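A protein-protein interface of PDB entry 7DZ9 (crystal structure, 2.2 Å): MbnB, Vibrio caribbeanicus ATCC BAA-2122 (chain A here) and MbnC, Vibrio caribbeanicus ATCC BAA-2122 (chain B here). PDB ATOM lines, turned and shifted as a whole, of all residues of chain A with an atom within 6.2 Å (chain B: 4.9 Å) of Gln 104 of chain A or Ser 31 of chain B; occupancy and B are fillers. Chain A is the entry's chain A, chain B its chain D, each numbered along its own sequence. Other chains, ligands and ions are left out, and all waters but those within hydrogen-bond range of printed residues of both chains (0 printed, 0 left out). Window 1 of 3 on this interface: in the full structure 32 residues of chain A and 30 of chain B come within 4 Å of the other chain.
Hydrophobic or aromatic side chains of chain B within 4 Å of the printed part of chain A: Leu 27 and Val 28. Among the printed residues, 5 pairs touch across the chains.
O of Leu 29 of chain B sits at hydrogen-bond distance from OG of Ser 32 of chain B, 3.1 Å away. OG of Ser 31 of chain B is in hydrogen-bond range of O of Val 28 of chain B, at 2.6 Å.
Among the printed residues, pairs that only touch across the chains: Pro 103 of chain A with Val 28 of chain B, Pro 103 of chain A with Ser 31 of chain B, Gln 104 of chain A with Ser 31 of chain B, Pro 103 of chain A with Ser 32 of chain B and Val 208 of chain A with Leu 27 of chain B.
Of the printed residues of chain B, Pro 103 of chain A touches Val 28, Ser 31 and Ser 32. Gln 104 of chain A touches one residue of chain B. Of the printed residues of chain B, Val 208 of chain A touches Leu 27 (3.9 Å). Of the printed residues of chain A, Val 28 of chain B touches Pro 103 (3.3 Å). Ser 31 of chain B touches just these residues of chain A: Pro 103 (3.4 Å) and Gln 104 (3.8 Å). Ser 34 of chain B touches none of the printed residues of chain A. The nearest printed residue of chain A that does not touch Val 28 of chain B is Gln 104 of chain A (4.2 Å).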
ATOM      1  N   LYS A  94      24.238   8.881   0.205  1.00  0.00           N
ATOM      2  CA  LYS A  94      22.832   8.530   0.081  1.00  0.00           C
ATOM      3  C   LYS A  94      22.659   7.584  -1.101  1.00  0.00           C
ATOM      4  O   LYS A  94      23.070   7.905  -2.223  1.00  0.00           O
ATOM      5  CB  LYS A  94      21.986   9.792  -0.099  1.00  0.00           C
ATOM      6  CG  LYS A  94      20.541   9.537  -0.434  1.00  0.00           C
ATOM      7  CD  LYS A  94      19.917  10.809  -0.927  1.00  0.00           C
ATOM      8  CE  LYS A  94      18.771  11.227  -0.036  1.00  0.00           C
ATOM      9  NZ  LYS A  94      19.257  11.696   1.275  1.00  0.00           N
ATOM     10  N   PHE A  95      21.996   6.445  -0.857  1.00  0.00           N
ATOM     11  CA  PHE A  95      21.925   5.363  -1.825  1.00  0.00           C
ATOM     12  C   PHE A  95      20.499   5.028  -2.251  1.00  0.00           C
ATOM     13  O   PHE A  95      20.317   4.300  -3.234  1.00  0.00           O
ATOM     14  CB  PHE A  95      22.576   4.084  -1.260  1.00  0.00           C
ATOM     15  CG  PHE A  95      24.076   4.194  -0.980  1.00  0.00           C
ATOM     16  CD1 PHE A  95      24.542   4.700   0.229  1.00  0.00           C
ATOM     17  CD2 PHE A  95      25.009   3.741  -1.905  1.00  0.00           C
ATOM     18  CE1 PHE A  95      25.914   4.767   0.503  1.00  0.00           C
ATOM     19  CE2 PHE A  95      26.387   3.804  -1.637  1.00  0.00           C
ATOM     20  CZ  PHE A  95      26.830   4.310  -0.427  1.00  0.00           C
ATOM     21  N   LEU A 102      19.371   4.284  -5.883  1.00  0.00           N
ATOM     22  CA  LEU A 102      19.966   5.238  -6.805  1.00  0.00           C
ATOM     23  C   LEU A 102      21.093   4.592  -7.603  1.00  0.00           C
ATOM     24  O   LEU A 102      21.763   3.667  -7.129  1.00  0.00           O
ATOM     25  CB  LEU A 102      20.499   6.444  -6.051  1.00  0.00           C
ATOM     26  CG  LEU A 102      19.376   7.119  -5.278  1.00  0.00           C
ATOM     27  CD1 LEU A 102      19.894   8.196  -4.300  1.00  0.00           C
ATOM     28  CD2 LEU A 102      18.343   7.663  -6.299  1.00  0.00           C
ATOM     29  N   PRO A 103      21.305   5.039  -8.840  1.00  0.00           N
ATOM     30  CA  PRO A 103      22.410   4.488  -9.628  1.00  0.00           C
ATOM     31  C   PRO A 103      23.761   5.053  -9.236  1.00  0.00           C
ATOM     32  O   PRO A 103      24.780   4.565  -9.740  1.00  0.00           O
ATOM     33  CB  PRO A 103      22.038   4.871 -11.066  1.00  0.00           C
ATOM     34  CG  PRO A 103      21.215   6.067 -10.945  1.00  0.00           C
ATOM     35  CD  PRO A 103      20.533   6.049  -9.584  1.00  0.00           C
ATOM     36  N   GLN A 104      23.793   6.093  -8.401  1.00  0.00           N
ATOM     37  CA  GLN A 104      25.021   6.694  -7.897  1.00  0.00           C
ATOM     38  C   GLN A 104      24.818   7.038  -6.428  1.00  0.00           C
ATOM     39  O   GLN A 104      23.687   7.226  -5.971  1.00  0.00           O
ATOM     40  CB  GLN A 104      25.390   7.984  -8.654  1.00  0.00           C
ATOM     41  CG  GLN A 104      25.584   7.833 -10.137  1.00  0.00           C
ATOM     42  CD  GLN A 104      27.054   7.671 -10.472  1.00  0.00           C
ATOM     43  OE1 GLN A 104      27.768   8.652 -10.640  1.00  0.00           O
ATOM     44  NE2 GLN A 104      27.521   6.429 -10.508  1.00  0.00           N
ATOM     45  N   MET A 105      25.925   7.176  -5.705  1.00  0.00           N
ATOM     46  CA  MET A 105      25.895   7.668  -4.332  1.00  0.00           C
ATOM     47  C   MET A 105      25.734   9.186  -4.363  1.00  0.00           C
ATOM     48  O   MET A 105      26.595   9.894  -4.897  1.00  0.00           O
ATOM     49  CB  MET A 105      27.179   7.268  -3.588  1.00  0.00           C
ATOM     50  CG  MET A 105      27.163   7.508  -2.056  1.00  0.00           C
ATOM     51  SD  MET A 105      28.748   7.115  -1.198  1.00  0.00           S
ATOM     52  CE  MET A 105      29.713   8.558  -1.604  1.00  0.00           C
ATOM     53  N   LEU A 106      24.653   9.687  -3.774  1.00  0.00           N
ATOM     54  CA  LEU A 106      24.363  11.116  -3.795  1.00  0.00           C
ATOM     55  C   LEU A 106      24.715  11.746  -2.452  1.00  0.00           C
ATOM     56  O   LEU A 106      24.907  11.055  -1.450  1.00  0.00           O
ATOM     57  CB  LEU A 106      22.892  11.369  -4.135  1.00  0.00           C
ATOM     58  CG  LEU A 106      22.536  11.461  -5.625  1.00  0.00           C
ATOM     59  CD1 LEU A 106      23.323  10.501  -6.495  1.00  0.00           C
ATOM     60  CD2 LEU A 106      21.054  11.233  -5.838  1.00  0.00           C
ATOM     61  N   VAL A 208      32.638  16.645 -12.018  1.00  0.00           N
ATOM     62  CA  VAL A 208      32.233  15.286 -11.667  1.00  0.00           C
ATOM     63  C   VAL A 208      33.452  14.551 -11.106  1.00  0.00           C
ATOM     64  O   VAL A 208      34.541  14.606 -11.690  1.00  0.00           O
ATOM     65  CB  VAL A 208      31.650  14.545 -12.886  1.00  0.00           C
ATOM     66  CG1 VAL A 208      31.014  13.204 -12.463  1.00  0.00           C
ATOM     67  CG2 VAL A 208      30.632  15.431 -13.631  1.00  0.00           C
ATOM     68  N   LEU B  27      22.502  13.074 -15.934  1.00  0.00           N
ATOM     69  CA  LEU B  27      23.772  12.383 -15.782  1.00  0.00           C
ATOM     70  C   LEU B  27      23.612  11.127 -14.920  1.00  0.00           C
ATOM     71  O   LEU B  27      24.030  10.037 -15.319  1.00  0.00           O
ATOM     72  CB  LEU B  27      24.811  13.341 -15.190  1.00  0.00           C
ATOM     73  CG  LEU B  27      26.236  12.791 -15.196  1.00  0.00           C
ATOM     74  CD1 LEU B  27      26.660  12.521 -16.623  1.00  0.00           C
ATOM     75  CD2 LEU B  27      27.181  13.750 -14.505  1.00  0.00           C
ATOM     76  N   VAL B  28      22.980  11.262 -13.750  1.00  0.00           N
ATOM     77  CA  VAL B  28      22.768  10.121 -12.851  1.00  0.00           C
ATOM     78  C   VAL B  28      21.951   9.037 -13.544  1.00  0.00           C
ATOM     79  O   VAL B  28      22.322   7.859 -13.546  1.00  0.00           O
ATOM     80  CB  VAL B  28      22.097  10.581 -11.546  1.00  0.00           C
ATOM     81  CG1 VAL B  28      21.775   9.395 -10.688  1.00  0.00           C
ATOM     82  CG2 VAL B  28      23.016  11.518 -10.782  1.00  0.00           C
ATOM     83  N   LEU B  29      20.851   9.426 -14.186  1.00  0.00           N
ATOM     84  CA  LEU B  29      20.060   8.462 -14.946  1.00  0.00           C
ATOM     85  C   LEU B  29      20.883   7.838 -16.066  1.00  0.00           C
ATOM     86  O   LEU B  29      20.731   6.649 -16.374  1.00  0.00           O
ATOM     87  CB  LEU B  29      18.821   9.131 -15.525  1.00  0.00           C
ATOM     88  CG  LEU B  29      17.677   9.293 -14.515  1.00  0.00           C
ATOM     89  CD1 LEU B  29      16.528  10.115 -15.087  1.00  0.00           C
ATOM     90  CD2 LEU B  29      17.208   7.940 -14.025  1.00  0.00           C
ATOM     91  N   GLN B  30      21.771   8.596 -16.697  1.00  0.00           N
ATOM     92  CA  GLN B  30      22.552   8.062 -17.845  1.00  0.00           C
ATOM     93  C   GLN B  30      23.453   6.915 -17.378  1.00  0.00           C
ATOM     94  O   GLN B  30      23.706   6.002 -18.163  1.00  0.00           O
ATOM     95  CB  GLN B  30      23.346   9.167 -18.541  1.00  0.00           C
ATOM     96  CG  GLN B  30      24.283   8.687 -19.639  1.00  0.00           C
ATOM     97  CD  GLN B  30      23.566   8.079 -20.818  1.00  0.00           C
ATOM     98  OE1 GLN B  30      23.858   6.964 -21.239  1.00  0.00           O
ATOM     99  NE2 GLN B  30      22.611   8.816 -21.359  1.00  0.00           N
ATOM    100  N   SER B  31      23.901   6.975 -16.129  1.00  0.00           N
ATOM    101  CA  SER B  31      24.812   5.931 -15.645  1.00  0.00           C
ATOM    102  C   SER B  31      24.160   4.554 -15.649  1.00  0.00           C
ATOM    103  O   SER B  31      24.814   3.565 -15.986  1.00  0.00           O
ATOM    104  CB  SER B  31      25.345   6.259 -14.256  1.00  0.00           C
ATOM    105  OG  SER B  31      24.323   6.185 -13.285  1.00  0.00           O
ATOM    106  N   SER B  32      22.900   4.455 -15.220  1.00  0.00           N
ATOM    107  CA  SER B  32      22.228   3.160 -15.228  1.00  0.00           C
ATOM    108  C   SER B  32      21.884   2.719 -16.651  1.00  0.00           C
ATOM    109  O   SER B  32      21.916   1.519 -16.946  1.00  0.00           O
ATOM    110  CB  SER B  32      20.989   3.197 -14.322  1.00  0.00           C
ATOM    111  OG  SER B  32      20.016   4.147 -14.742  1.00  0.00           O
ATOM    112  N   GLN B  33      21.588   3.655 -17.557  1.00  0.00           N
ATOM    113  CA  GLN B  33      21.374   3.250 -18.944  1.00  0.00           C
ATOM    114  C   GLN B  33      22.662   2.721 -19.572  1.00  0.00           C
ATOM    115  O   GLN B  33      22.632   1.731 -20.321  1.00  0.00           O
ATOM    116  CB  GLN B  33      20.825   4.407 -19.794  1.00  0.00           C
ATOM    117  CG  GLN B  33      20.375   3.901 -21.215  1.00  0.00           C
ATOM    118  CD  GLN B  33      20.338   4.993 -22.269  1.00  0.00           C
ATOM    119  OE1 GLN B  33      21.085   5.969 -22.195  1.00  0.00           O
ATOM    120  NE2 GLN B  33      19.454   4.837 -23.257  1.00  0.00           N
ATOM    121  N   SER B  34      23.786   3.401 -19.327  1.00  0.00           N
ATOM    122  CA  SER B  34      25.073   2.945 -19.854  1.00  0.00           C
ATOM    123  C   SER B  34      25.401   1.531 -19.397  1.00  0.00           C
ATOM    124  O   SER B  34      25.925   0.722 -20.174  1.00  0.00           O
ATOM    125  CB  SER B  34      26.173   3.923 -19.464  1.00  0.00           C
ATOM    126  OG  SER B  34      25.914   5.156 -20.108  1.00  0.00           O
ATOM    127  N   LEU B  35      25.149   1.231 -18.130  1.00  0.00           N
ATOM    128  CA  LEU B  35      25.419  -0.116 -17.642  1.00  0.00           C
ATOM    129  C   LEU B  35      24.673  -1.151 -18.476  1.00  0.00           C
ATOM    130  O   LEU B  35      25.258  -2.126 -18.953  1.00  0.00           O
ATOM    131  CB  LEU B  35      25.026  -0.203 -16.166  1.00  0.00           C
ATOM    132  CG  LEU B  35      25.042  -1.530 -15.409  1.00  0.00           C
ATOM    133  CD1 LEU B  35      25.402  -1.281 -13.967  1.00  0.00           C
ATOM    134  CD2 LEU B  35      23.681  -2.200 -15.450  1.00  0.00           C
